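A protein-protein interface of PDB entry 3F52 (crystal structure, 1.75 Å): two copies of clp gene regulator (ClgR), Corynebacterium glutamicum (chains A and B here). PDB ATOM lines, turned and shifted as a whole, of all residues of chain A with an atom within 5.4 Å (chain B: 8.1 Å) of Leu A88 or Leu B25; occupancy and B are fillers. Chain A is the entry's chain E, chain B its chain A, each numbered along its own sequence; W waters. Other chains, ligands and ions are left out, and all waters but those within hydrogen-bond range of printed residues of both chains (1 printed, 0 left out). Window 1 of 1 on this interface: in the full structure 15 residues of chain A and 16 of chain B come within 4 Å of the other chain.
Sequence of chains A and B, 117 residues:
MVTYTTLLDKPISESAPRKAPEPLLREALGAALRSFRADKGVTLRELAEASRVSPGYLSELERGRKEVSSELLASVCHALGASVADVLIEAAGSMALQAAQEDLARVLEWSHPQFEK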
ATOM      1  N   LEU A  25     -31.112 -11.576   3.809  1.00  0.00           N
ATOM      2  CA  LEU A  25     -29.841 -12.286   3.629  1.00  0.00           C
ATOM      3  C   LEU A  25     -29.168 -12.573   4.963  1.00  0.00           C
ATOM      4  O   LEU A  25     -28.676 -13.685   5.178  1.00  0.00           O
ATOM      5  CB  LEU A  25     -28.883 -11.490   2.728  1.00  0.00           C
ATOM      6  CG  LEU A  25     -27.515 -12.191   2.513  1.00  0.00           C
ATOM      7  CD1 LEU A  25     -27.661 -13.657   1.983  1.00  0.00           C
ATOM      8  CD2 LEU A  25     -26.633 -11.351   1.598  1.00  0.00           C
ATOM      9  N   LEU A  29     -27.941 -16.168   6.055  1.00  0.00           N
ATOM     10  CA  LEU A  29     -26.516 -16.371   6.307  1.00  0.00           C
ATOM     11  C   LEU A  29     -26.248 -16.761   7.754  1.00  0.00           C
ATOM     12  O   LEU A  29     -25.420 -17.647   8.033  1.00  0.00           O
ATOM     13  CB  LEU A  29     -25.767 -15.083   5.993  1.00  0.00           C
ATOM     14  CG  LEU A  29     -24.350 -14.981   5.464  1.00  0.00           C
ATOM     15  CD1 LEU A  29     -24.195 -15.852   4.222  1.00  0.00           C
ATOM     16  CD2 LEU A  29     -23.999 -13.483   5.115  1.00  0.00           C
ATOM     17  N   SER A  70     -17.578  -8.402   4.496  1.00  0.00           N
ATOM     18  CA  SER A  70     -17.079  -9.572   3.766  1.00  0.00           C
ATOM     19  C   SER A  70     -15.839 -10.169   4.448  1.00  0.00           C
ATOM     20  O   SER A  70     -15.692 -11.384   4.484  1.00  0.00           O
ATOM     21  CB  SER A  70     -16.749  -9.217   2.316  1.00  0.00           C
ATOM     22  OG  SER A  70     -17.940  -8.821   1.646  1.00  0.00           O
ATOM     23  N   LEU A  73     -16.851 -12.044   7.627  1.00  0.00           N
ATOM     24  CA  LEU A  73     -17.450 -13.308   7.233  1.00  0.00           C
ATOM     25  C   LEU A  73     -16.378 -14.321   6.816  1.00  0.00           C
ATOM     26  O   LEU A  73     -16.453 -15.504   7.160  1.00  0.00           O
ATOM     27  CB  LEU A  73     -18.476 -13.108   6.104  1.00  0.00           C
ATOM     28  CG  LEU A  73     -19.108 -14.393   5.556  1.00  0.00           C
ATOM     29  CD1 LEU A  73     -19.896 -15.160   6.645  1.00  0.00           C
ATOM     30  CD2 LEU A  73     -20.018 -14.035   4.379  1.00  0.00           C
ATOM     31  N   SER A  83     -15.744 -22.917   3.371  1.00  0.00           N
ATOM     32  CA  SER A  83     -15.627 -21.817   2.398  1.00  0.00           C
ATOM     33  C   SER A  83     -16.823 -20.882   2.515  1.00  0.00           C
ATOM     34  O   SER A  83     -17.909 -21.303   2.922  1.00  0.00           O
ATOM     35  CB  SER A  83     -15.476 -22.311   0.958  1.00  0.00           C
ATOM     36  OG  SER A  83     -16.657 -22.958   0.509  1.00  0.00           O
ATOM     37  N   VAL A  84     -16.626 -19.607   2.176  1.00  0.00           N
ATOM     38  CA  VAL A  84     -17.750 -18.659   2.144  1.00  0.00           C
ATOM     39  C   VAL A  84     -18.780 -19.130   1.076  1.00  0.00           C
ATOM     40  O   VAL A  84     -19.982 -19.008   1.273  1.00  0.00           O
ATOM     41  CB  VAL A  84     -17.270 -17.208   1.877  1.00  0.00           C
ATOM     42  CG1 VAL A  84     -18.458 -16.265   1.707  1.00  0.00           C
ATOM     43  CG2 VAL A  84     -16.335 -16.733   3.024  1.00  0.00           C
ATOM     44  N   ALA A  85     -18.287 -19.658  -0.041  1.00  0.00           N
ATOM     45  CA  ALA A  85     -19.146 -20.161  -1.117  1.00  0.00           C
ATOM     46  C   ALA A  85     -20.126 -21.206  -0.583  1.00  0.00           C
ATOM     47  O   ALA A  85     -21.310 -21.157  -0.886  1.00  0.00           O
ATOM     48  CB  ALA A  85     -18.297 -20.750  -2.267  1.00  0.00           C
ATOM     49  N   ASP A  86     -19.635 -22.139   0.229  1.00  0.00           N
ATOM     50  CA  ASP A  86     -20.492 -23.201   0.760  1.00  0.00           C
ATOM     51  C   ASP A  86     -21.503 -22.655   1.780  1.00  0.00           C
ATOM     52  O   ASP A  86     -22.662 -23.067   1.805  1.00  0.00           O
ATOM     53  CB  ASP A  86     -19.662 -24.341   1.381  1.00  0.00           C
ATOM     54  CG  ASP A  86     -18.938 -25.202   0.336  1.00  0.00           C
ATOM     55  OD1 ASP A  86     -19.265 -25.151  -0.889  1.00  0.00           O
ATOM     56  OD2 ASP A  86     -18.020 -25.957   0.767  1.00  0.00           O
ATOM     57  N   VAL A  87     -21.064 -21.722   2.625  1.00  0.00           N
ATOM     58  CA  VAL A  87     -21.973 -21.063   3.564  1.00  0.00           C
ATOM     59  C   VAL A  87     -23.042 -20.276   2.804  1.00  0.00           C
ATOM     60  O   VAL A  87     -24.215 -20.330   3.152  1.00  0.00           O
ATOM     61  CB  VAL A  87     -21.187 -20.174   4.567  1.00  0.00           C
ATOM     62  CG1 VAL A  87     -22.129 -19.351   5.439  1.00  0.00           C
ATOM     63  CG2 VAL A  87     -20.297 -21.092   5.428  1.00  0.00           C
ATOM     64  N   LEU A  88     -22.636 -19.571   1.756  1.00  0.00           N
ATOM     65  CA  LEU A  88     -23.587 -18.790   0.945  1.00  0.00           C
ATOM     66  C   LEU A  88     -24.634 -19.662   0.213  1.00  0.00           C
ATOM     67  O   LEU A  88     -25.828 -19.336   0.183  1.00  0.00           O
ATOM     68  CB  LEU A  88     -22.838 -17.909  -0.051  1.00  0.00           C
ATOM     69  CG  LEU A  88     -23.648 -16.861  -0.820  1.00  0.00           C
ATOM     70  CD1 LEU A  88     -24.321 -15.880   0.154  1.00  0.00           C
ATOM     71  CD2 LEU A  88     -22.719 -16.095  -1.776  1.00  0.00           C
ATOM     72  N   ILE A  89     -24.205 -20.771  -0.370  1.00  0.00           N
ATOM     73  CA  ILE A  89     -25.163 -21.632  -1.012  1.00  0.00           C
ATOM     74  C   ILE A  89     -26.126 -22.251   0.034  1.00  0.00           C
ATOM     75  O   ILE A  89     -27.322 -22.375  -0.220  1.00  0.00           O
ATOM     76  CB  ILE A  89     -24.485 -22.675  -1.952  1.00  0.00           C
ATOM     77  CG1 ILE A  89     -25.490 -23.206  -2.980  1.00  0.00           C
ATOM     78  CG2 ILE A  89     -23.846 -23.780  -1.167  1.00  0.00           C
ATOM     79  CD1 ILE A  89     -25.781 -22.178  -4.067  1.00  0.00           C
ATOM     80  N   GLU A  90     -25.627 -22.604   1.220  1.00  0.00           N
ATOM     81  CA  GLU A  90     -26.523 -23.070   2.283  1.00  0.00           C
ATOM     82  C   GLU A  90     -27.558 -21.983   2.661  1.00  0.00           C
ATOM     83  O   GLU A  90     -28.757 -22.278   2.837  1.00  0.00           O
ATOM     84  CB  GLU A  90     -25.730 -23.495   3.532  1.00  0.00           C
ATOM     85  CG  GLU A  90     -26.570 -24.183   4.628  1.00  0.00           C
ATOM     86  CD  GLU A  90     -27.308 -25.430   4.117  1.00  0.00           C
ATOM     87  OE1 GLU A  90     -26.700 -26.254   3.375  1.00  0.00           O
ATOM     88  OE2 GLU A  90     -28.493 -25.618   4.486  1.00  0.00           O
ATOM     89  N   ALA A  91     -27.090 -20.743   2.763  1.00  0.00           N
ATOM     90  CA  ALA A  91     -27.949 -19.602   3.072  1.00  0.00           C
ATOM     91  C   ALA A  91     -29.079 -19.456   2.045  1.00  0.00           C
ATOM     92  O   ALA A  91     -30.224 -19.136   2.391  1.00  0.00           O
ATOM     93  CB  ALA A  91     -27.113 -18.352   3.121  1.00  0.00           C
ATOM     94  N   ALA A  92     -28.809 -19.764   0.771  1.00  0.00           N
ATOM     95  CA  ALA A  92     -29.860 -19.747  -0.248  1.00  0.00           C
ATOM     96  C   ALA A  92     -31.006 -20.685   0.122  1.00  0.00           C
ATOM     97  O   ALA A  92     -32.162 -20.385  -0.176  1.00  0.00           O
ATOM     98  CB  ALA A  92     -29.286 -20.084  -1.682  1.00  0.00           C
ATOM     99  N   GLU B  22     -10.233 -16.718  -2.068  1.00  0.00           N
ATOM    100  CA  GLU B  22     -11.697 -16.690  -2.305  1.00  0.00           C
ATOM    101  C   GLU B  22     -12.084 -15.232  -2.529  1.00  0.00           C
ATOM    102  O   GLU B  22     -11.618 -14.364  -1.788  1.00  0.00           O
ATOM    103  CB  GLU B  22     -12.440 -17.268  -1.086  1.00  0.00           C
ATOM    104  CG  GLU B  22     -13.954 -17.469  -1.249  1.00  0.00           C
ATOM    105  CD  GLU B  22     -14.521 -18.645  -0.411  1.00  0.00           C
ATOM    106  OE1 GLU B  22     -14.071 -18.865   0.745  1.00  0.00           O
ATOM    107  OE2 GLU B  22     -15.427 -19.360  -0.920  1.00  0.00           O
ATOM    108  N   PRO B  23     -12.909 -14.942  -3.559  1.00  0.00           N
ATOM    109  CA  PRO B  23     -13.391 -13.562  -3.644  1.00  0.00           C
ATOM    110  C   PRO B  23     -14.132 -13.172  -2.359  1.00  0.00           C
ATOM    111  O   PRO B  23     -14.625 -14.047  -1.620  1.00  0.00           O
ATOM    112  CB  PRO B  23     -14.393 -13.606  -4.816  1.00  0.00           C
ATOM    113  CG  PRO B  23     -13.967 -14.781  -5.644  1.00  0.00           C
ATOM    114  CD  PRO B  23     -13.436 -15.784  -4.655  1.00  0.00           C
ATOM    115  N   LEU B  24     -14.204 -11.874  -2.096  1.00  0.00           N
ATOM    116  CA  LEU B  24     -15.055 -11.361  -1.030  1.00  0.00           C
ATOM    117  C   LEU B  24     -16.527 -11.511  -1.381  1.00  0.00           C
ATOM    118  O   LEU B  24     -16.915 -11.374  -2.548  1.00  0.00           O
ATOM    119  CB  LEU B  24     -14.765  -9.875  -0.790  1.00  0.00           C
ATOM    120  CG  LEU B  24     -13.327  -9.615  -0.338  1.00  0.00           C
ATOM    121  CD1 LEU B  24     -13.039  -8.137  -0.436  1.00  0.00           C
ATOM    122  CD2 LEU B  24     -13.147 -10.099   1.095  1.00  0.00           C
ATOM    123  N   LEU B  25     -17.354 -11.739  -0.358  1.00  0.00           N
ATOM    124  CA  LEU B  25     -18.791 -11.778  -0.552  1.00  0.00           C
ATOM    125  C   LEU B  25     -19.312 -10.596  -1.379  1.00  0.00           C
ATOM    126  O   LEU B  25     -20.113 -10.796  -2.327  1.00  0.00           O
ATOM    127  CB  LEU B  25     -19.509 -11.841   0.785  1.00  0.00           C
ATOM    128  CG  LEU B  25     -21.053 -11.835   0.672  1.00  0.00           C
ATOM    129  CD1 LEU B  25     -21.620 -13.102  -0.038  1.00  0.00           C
ATOM    130  CD2 LEU B  25     -21.626 -11.656   2.067  1.00  0.00           C
ATOM    131  N   ARG B  26     -18.895  -9.362  -1.035  1.00  0.00           N
ATOM    132  CA  ARG B  26     -19.420  -8.214  -1.767  1.00  0.00           C
ATOM    133  C   ARG B  26     -19.060  -8.292  -3.261  1.00  0.00           C
ATOM    134  O   ARG B  26     -19.846  -7.855  -4.100  1.00  0.00           O
ATOM    135  CB  ARG B  26     -18.972  -6.886  -1.111  1.00  0.00           C
ATOM    136  CG  ARG B  26     -17.462  -6.616  -1.144  1.00  0.00           C
ATOM    137  CD  ARG B  26     -17.223  -5.233  -0.514  1.00  0.00           C
ATOM    138  NE  ARG B  26     -15.795  -4.932  -0.442  1.00  0.00           N
ATOM    139  CZ  ARG B  26     -15.015  -5.177   0.605  1.00  0.00           C
ATOM    140  NH1 ARG B  26     -13.731  -4.895   0.534  1.00  0.00           N
ATOM    141  NH2 ARG B  26     -15.489  -5.726   1.717  1.00  0.00           N
ATOM    142  N   GLU B  27     -17.880  -8.843  -3.573  1.00  0.00           N
ATOM    143  CA  GLU B  27     -17.441  -8.966  -4.966  1.00  0.00           C
ATOM    144  C   GLU B  27     -18.331  -9.962  -5.712  1.00  0.00           C
ATOM    145  O   GLU B  27     -18.766  -9.703  -6.849  1.00  0.00           O
ATOM    146  CB  GLU B  27     -15.966  -9.353  -5.045  1.00  0.00           C
ATOM    147  CG  GLU B  27     -15.033  -8.177  -4.624  1.00  0.00           C
ATOM    148  CD  GLU B  27     -13.610  -8.596  -4.369  1.00  0.00           C
ATOM    149  OE1 GLU B  27     -13.322  -9.794  -4.205  1.00  0.00           O
ATOM    150  OE2 GLU B  27     -12.764  -7.687  -4.303  1.00  0.00           O
ATOM    151  N   ALA B  28     -18.640 -11.061  -5.034  1.00  0.00           N
ATOM    152  CA  ALA B  28     -19.459 -12.121  -5.606  1.00  0.00           C
ATOM    153  C   ALA B  28     -20.906 -11.641  -5.820  1.00  0.00           C
ATOM    154  O   ALA B  28     -21.505 -11.869  -6.888  1.00  0.00           O
ATOM    155  CB  ALA B  28     -19.424 -13.362  -4.704  1.00  0.00           C
ATOM    156  N   LEU B  29     -21.470 -10.993  -4.801  1.00  0.00           N
ATOM    157  CA  LEU B  29     -22.826 -10.488  -4.877  1.00  0.00           C
ATOM    158  C   LEU B  29     -22.966  -9.442  -5.960  1.00  0.00           C
ATOM    159  O   LEU B  29     -23.915  -9.448  -6.748  1.00  0.00           O
ATOM    160  CB  LEU B  29     -23.243  -9.890  -3.521  1.00  0.00           C
ATOM    161  CG  LEU B  29     -23.496 -10.857  -2.366  1.00  0.00           C
ATOM    162  CD1 LEU B  29     -23.852 -10.039  -1.112  1.00  0.00           C
ATOM    163  CD2 LEU B  29     -24.626 -11.859  -2.701  1.00  0.00           C
ATOM    164  N   GLY B  30     -21.989  -8.555  -6.033  1.00  0.00           N
ATOM    165  CA  GLY B  30     -22.057  -7.478  -7.006  1.00  0.00           C
ATOM    166  C   GLY B  30     -21.949  -7.995  -8.442  1.00  0.00           C
ATOM    167  O   GLY B  30     -22.664  -7.535  -9.340  1.00  0.00           O
ATOM    168  N   ALA B  31     -21.051  -8.935  -8.652  1.00  0.00           N
ATOM    169  CA  ALA B  31     -20.907  -9.552  -9.970  1.00  0.00           C
ATOM    170  C   ALA B  31     -22.178 -10.305 -10.375  1.00  0.00           C
ATOM    171  O   ALA B  31     -22.550 -10.305 -11.549  1.00  0.00           O
ATOM    172  CB  ALA B  31     -19.715 -10.455  -9.981  1.00  0.00           C
ATOM    173  N   ALA B  32     -22.848 -10.939  -9.401  1.00  0.00           N
ATOM    174  CA  ALA B  32     -24.120 -11.632  -9.671  1.00  0.00           C
ATOM    175  C   ALA B  32     -25.205 -10.613 -10.062  1.00  0.00           C
ATOM    176  O   ALA B  32     -25.964 -10.822 -11.028  1.00  0.00           O
ATOM    177  CB  ALA B  32     -24.560 -12.470  -8.461  1.00  0.00           C
ATOM    178  N   LEU B  61     -21.349  -1.042  -6.158  1.00  0.00           N
ATOM    179  CA  LEU B  61     -21.880  -2.311  -5.612  1.00  0.00           C
ATOM    180  C   LEU B  61     -21.571  -3.484  -6.571  1.00  0.00           C
ATOM    181  O   LEU B  61     -21.062  -4.530  -6.169  1.00  0.00           O
ATOM    182  CB  LEU B  61     -23.380  -2.169  -5.376  1.00  0.00           C
ATOM    183  CG  LEU B  61     -23.825  -1.217  -4.266  1.00  0.00           C
ATOM    184  CD1 LEU B  61     -25.314  -0.966  -4.411  1.00  0.00           C
ATOM    185  CD2 LEU B  61     -23.493  -1.716  -2.841  1.00  0.00           C
ATOM    186  N   GLY B  64     -18.146  -4.689  -6.299  1.00  0.00           N
ATOM    187  CA  GLY B  64     -17.712  -5.114  -4.959  1.00  0.00           C
ATOM    188  C   GLY B  64     -16.941  -4.063  -4.177  1.00  0.00           C
ATOM    189  O   GLY B  64     -16.140  -4.403  -3.303  1.00  0.00           O
ATOM    190  N   LYS B  66     -18.306  -1.871  -2.216  1.00  0.00           N
ATOM    191  CA  LYS B  66     -19.100  -1.511  -1.053  1.00  0.00           C
ATOM    192  C   LYS B  66     -19.848  -2.750  -0.652  1.00  0.00           C
ATOM    193  O   LYS B  66     -20.180  -3.553  -1.506  1.00  0.00           O
ATOM    194  CB  LYS B  66     -20.184  -0.494  -1.437  1.00  0.00           C
ATOM    195  CG  LYS B  66     -19.678   0.742  -2.123  1.00  0.00           C
ATOM    196  CD  LYS B  66     -19.255   1.724  -1.129  1.00  0.00           C
ATOM    197  CE  LYS B  66     -19.237   3.078  -1.757  1.00  0.00           C
ATOM    198  NZ  LYS B  66     -18.229   3.808  -1.039  1.00  0.00           N
ATOM    199  N   GLU B  67     -20.135  -2.902   0.639  1.00  0.00           N
ATOM    200  CA  GLU B  67     -20.979  -4.022   1.046  1.00  0.00           C
ATOM    201  C   GLU B  67     -22.380  -3.920   0.466  1.00  0.00           C
ATOM    202  O   GLU B  67     -22.931  -2.820   0.286  1.00  0.00           O
ATOM    203  CB  GLU B  67     -21.025  -4.165   2.568  1.00  0.00           C
ATOM    204  CG  GLU B  67     -19.682  -4.383   3.231  1.00  0.00           C
ATOM    205  CD  GLU B  67     -19.038  -5.754   2.953  1.00  0.00           C
ATOM    206  OE1 GLU B  67     -19.674  -6.707   2.426  1.00  0.00           O
ATOM    207  OE2 GLU B  67     -17.861  -5.860   3.313  1.00  0.00           O
ATOM    208  N   VAL B  68     -22.934  -5.079   0.140  1.00  0.00           N
ATOM    209  CA  VAL B  68     -24.303  -5.164  -0.383  1.00  0.00           C
ATOM    210  C   VAL B  68     -25.155  -5.654   0.788  1.00  0.00           C
ATOM    211  O   VAL B  68     -25.165  -6.862   1.112  1.00  0.00           O
ATOM    212  CB  VAL B  68     -24.407  -6.141  -1.583  1.00  0.00           C
ATOM    213  CG1 VAL B  68     -25.828  -6.064  -2.234  1.00  0.00           C
ATOM    214  CG2 VAL B  68     -23.300  -5.878  -2.631  1.00  0.00           C
ATOM    215  N   LEU B  73     -29.821  -5.432  -1.152  1.00  0.00           N
ATOM    216  CA  LEU B  73     -29.900  -6.597  -2.031  1.00  0.00           C
ATOM    217  C   LEU B  73     -31.358  -6.904  -2.388  1.00  0.00           C
ATOM    218  O   LEU B  73     -31.683  -7.108  -3.555  1.00  0.00           O
ATOM    219  CB  LEU B  73     -29.238  -7.823  -1.389  1.00  0.00           C
ATOM    220  CG  LEU B  73     -29.206  -9.075  -2.273  1.00  0.00           C
ATOM    221  CD1 LEU B  73     -28.435  -8.848  -3.582  1.00  0.00           C
ATOM    222  CD2 LEU B  73     -28.605 -10.257  -1.476  1.00  0.00           C
ATOM    223  N   VAL B  84     -33.768 -13.092  -4.707  1.00  0.00           N
ATOM    224  CA  VAL B  84     -32.505 -12.974  -4.004  1.00  0.00           C
ATOM    225  C   VAL B  84     -31.816 -14.355  -3.980  1.00  0.00           C
ATOM    226  O   VAL B  84     -30.617 -14.429  -4.202  1.00  0.00           O
ATOM    227  CB  VAL B  84     -32.702 -12.459  -2.547  1.00  0.00           C
ATOM    228  CG1 VAL B  84     -31.381 -12.523  -1.756  1.00  0.00           C
ATOM    229  CG2 VAL B  84     -33.197 -10.989  -2.550  1.00  0.00           C
ATOM    230  N   ALA B  85     -32.562 -15.439  -3.725  1.00  0.00           N
ATOM    231  CA  ALA B  85     -31.911 -16.758  -3.653  1.00  0.00           C
ATOM    232  C   ALA B  85     -31.135 -17.094  -4.922  1.00  0.00           C
ATOM    233  O   ALA B  85     -30.040 -17.636  -4.856  1.00  0.00           O
ATOM    234  CB  ALA B  85     -32.931 -17.873  -3.348  1.00  0.00           C
ATOM    235  N   VAL B  87     -29.762 -14.954  -6.997  1.00  0.00           N
ATOM    236  CA  VAL B  87     -28.559 -14.136  -7.032  1.00  0.00           C
ATOM    237  C   VAL B  87     -27.490 -14.733  -6.099  1.00  0.00           C
ATOM    238  O   VAL B  87     -26.337 -14.788  -6.467  1.00  0.00           O
ATOM    239  CB  VAL B  87     -28.917 -12.642  -6.672  1.00  0.00           C
ATOM    240  CG1 VAL B  87     -27.656 -11.802  -6.418  1.00  0.00           C
ATOM    241  CG2 VAL B  87     -29.775 -12.050  -7.801  1.00  0.00           C
ATOM    242  N   LEU B  88     -27.906 -15.272  -4.946  1.00  0.00           N
ATOM    243  CA  LEU B  88     -26.965 -15.917  -4.035  1.00  0.00           C
ATOM    244  C   LEU B  88     -26.315 -17.164  -4.636  1.00  0.00           C
ATOM    245  O   LEU B  88     -25.115 -17.418  -4.441  1.00  0.00           O
ATOM    246  CB  LEU B  88     -27.664 -16.326  -2.744  1.00  0.00           C
ATOM    247  CG  LEU B  88     -28.355 -15.227  -1.935  1.00  0.00           C
ATOM    248  CD1 LEU B  88     -28.746 -15.831  -0.558  1.00  0.00           C
ATOM    249  CD2 LEU B  88     -27.419 -13.996  -1.805  1.00  0.00           C
ATOM    250  N   ILE B  89     -27.132 -17.956  -5.327  1.00  0.00           N
ATOM    251  CA  ILE B  89     -26.634 -19.163  -6.007  1.00  0.00           C
ATOM    252  C   ILE B  89     -25.564 -18.761  -7.044  1.00  0.00           C
ATOM    253  O   ILE B  89     -24.508 -19.406  -7.118  1.00  0.00           O
ATOM    254  CB  ILE B  89     -27.774 -19.954  -6.644  1.00  0.00           C
ATOM    255  CG1 ILE B  89     -28.628 -20.597  -5.532  1.00  0.00           C
ATOM    256  CG2 ILE B  89     -27.245 -21.011  -7.635  1.00  0.00           C
ATOM    257  CD1 ILE B  89     -29.985 -21.077  -6.039  1.00  0.00           C
ATOM    258  N   GLU B  90     -25.862 -17.740  -7.854  1.00  0.00           N
ATOM    259  CA  GLU B  90     -24.890 -17.228  -8.844  1.00  0.00           C
ATOM    260  C   GLU B  90     -23.581 -16.695  -8.191  1.00  0.00           C
ATOM    261  O   GLU B  90     -22.449 -17.007  -8.648  1.00  0.00           O
ATOM    262  CB  GLU B  90     -25.565 -16.135  -9.691  1.00  0.00           C
ATOM    263  CG  GLU B  90     -24.627 -15.406 -10.673  1.00  0.00           C
ATOM    264  CD  GLU B  90     -24.093 -16.307 -11.773  1.00  0.00           C
ATOM    265  OE1 GLU B  90     -24.618 -17.437 -11.954  1.00  0.00           O
ATOM    266  OE2 GLU B  90     -23.117 -15.889 -12.444  1.00  0.00           O
ATOM    267  N   ALA B  91     -23.748 -15.917  -7.119  1.00  0.00           N
ATOM    268  CA  ALA B  91     -22.633 -15.380  -6.342  1.00  0.00           C
ATOM    269  C   ALA B  91     -21.769 -16.519  -5.798  1.00  0.00           C
ATOM    270  O   ALA B  91     -20.544 -16.474  -5.925  1.00  0.00           O
ATOM    271  CB  ALA B  91     -23.154 -14.476  -5.188  1.00  0.00           C
ATOM    272  N   ALA B  92     -22.401 -17.573  -5.269  1.00  0.00           N
ATOM    273  CA  ALA B  92     -21.631 -18.664  -4.691  1.00  0.00           C
ATOM    274  C   ALA B  92     -20.848 -19.406  -5.779  1.00  0.00           C
ATOM    275  O   ALA B  92     -19.730 -19.864  -5.549  1.00  0.00           O
ATOM    276  CB  ALA B  92     -22.514 -19.640  -3.904  1.00  0.00           C
ATOM    277  N   GLY B  93     -21.453 -19.517  -6.960  1.00  0.00           N
ATOM    278  CA  GLY B  93     -20.806 -20.199  -8.100  1.00  0.00           C
ATOM    279  C   GLY B  93     -19.596 -19.432  -8.581  1.00  0.00           C
ATOM    280  O   GLY B  93     -18.596 -20.021  -8.975  1.00  0.00           O
ATOM    281  N   SER B  94     -19.666 -18.108  -8.530  1.00  0.00           N
ATOM    282  CA  SER B  94     -18.571 -17.300  -9.046  1.00  0.00           C
ATOM    283  C   SER B  94     -17.364 -17.363  -8.112  1.00  0.00           C
ATOM    284  O   SER B  94     -16.255 -17.040  -8.525  1.00  0.00           O
ATOM    285  CB  SER B  94     -19.046 -15.867  -9.195  1.00  0.00           C
ATOM    286  OG  SER B  94     -19.136 -15.292  -7.919  1.00  0.00           O
ATOM    287  N   MET B  95     -17.593 -17.761  -6.858  1.00  0.00           N
ATOM    288  CA  MET B  95     -16.570 -17.763  -5.804  1.00  0.00           C
ATOM    289  C   MET B  95     -15.774 -19.042  -5.707  1.00  0.00           C
ATOM    290  O   MET B  95     -14.658 -19.039  -5.183  1.00  0.00           O
ATOM    291  CB  MET B  95     -17.216 -17.573  -4.446  1.00  0.00           C
ATOM    292  CG  MET B  95     -17.835 -16.251  -4.272  1.00  0.00           C
ATOM    293  SD  MET B  95     -18.637 -16.234  -2.675  1.00  0.00           S
ATOM    294  CE  MET B  95     -17.316 -15.575  -1.673  1.00  0.00           C
HETATM  295  O   HOH W   1     -16.302 -12.711   2.066  1.00  0.00           O
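The side-chain hydroxyl (OG) of Ser B94 lies within hydrogen-bond range of the backbone carbonyl oxygen (O) of Ala B91 (2.7 Å). The backbone NH (N) of Leu B24 lies within hydrogen-bond range of the side-chain carboxylate (OE1) of Glu B27. The side-chain hydroxyl of Ser A83 is in hydrogen-bond range of the backbone NH of Asp A86 (3.1 Å). The side-chain carboxylate of Glu B67 is in salt-bridge range of the guanidinium group of Arg B26, 2.9 Å away. The guanidinium group (NE) of Arg B26 is in hydrogen-bond range of the backbone carbonyl oxygen (O) of Gly B64, 2.9 Å away.
Printed residues of chain B within 4 Å of Val A84: Glu B22 and Met B95. Leu A88 touches just these residues of chain B: Leu B25, Leu B88, Ala B91 and Ala B92. Printed residues of chain B within 4 Å of Ala A92: Ile B89. Printed residues of chain A within 4 Å of Glu B22: Ser A83, Val A84 and Ala A85. Leu B25 touches just these residues of chain A: Ser A70 (3.5 Å), Leu A73 (3.7 Å) and Leu A88 (3.6 Å). Of the printed residues of chain A, Met B95 touches Val A84 (3.6 Å). The nearest residue of chain A that does not touch Leu B25 is Leu A29 (4.3 Å). The nearest printed residue of chain A that does not touch Ile B89 is Leu A88 (5.8 Å).
The backbone NH (N) of Ser A70 lies within hydrogen-bond range of the side-chain carboxylate (OE2) of Glu B67, 2.8 Å away. The backbone NH of Val A84 lies within hydrogen-bond range of the side-chain carboxylate of Glu B22. N of Arg B26 lies within hydrogen-bond range of OG of Ser A70 (2.9 Å). The side-chain carboxylate of Glu B22 is in hydrogen-bond range of the backbone NH of Ala A85 (3.0 Å).
Water W1 lies within hydrogen-bond range of N of Leu B25 (2.8 Å) and O of Ser A70 (2.8 Å).
Leu A25 touches Leu B73, and with the chains exchanged Leu A73 touches Leu B25. Ala A85 touches Ala B92, but with the chains exchanged Ala A92 does not touch Ala B85 (4.1 Å). Leu B88 touches its own counterpart, Leu A88. Ile B89 touches its own counterpart, Ile A89. 11 positions are printed for both chains.
Among the printed residues, pairs that only touch across the chains: Ser A83 with Glu B22, Ser A70 with Leu B25, Leu A25 with Leu B88, Ile A89 with Ile B89, Ala A85 with Ala B92, Leu A88 with Leu B25, Val A84 with Met B95, Leu A73 with Leu B25, Ser A70 with Leu B24, Leu A88 with Ala B91, Leu A88 with Ala B92, Leu A25 with Leu B73, Leu A88 with Leu B88 and Ala A92 with Ile B89.
Of the 14 printed residues of chain A, 9 touch a printed residue of chain B. Hydrophobic or aromatic side chains of chain A that line the printed part of chain B: Leu A25, Leu A73, Val A84, Ala A85, Leu A88, Ile A89 and Ala A92. Along chain A the printed residues that touch a printed residue of chain B span positions 25 to 92. Along chain B the printed residues that touch a printed residue of chain A span positions 22 to 95. Among the printed residues, 18 pairs touch across the chains.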
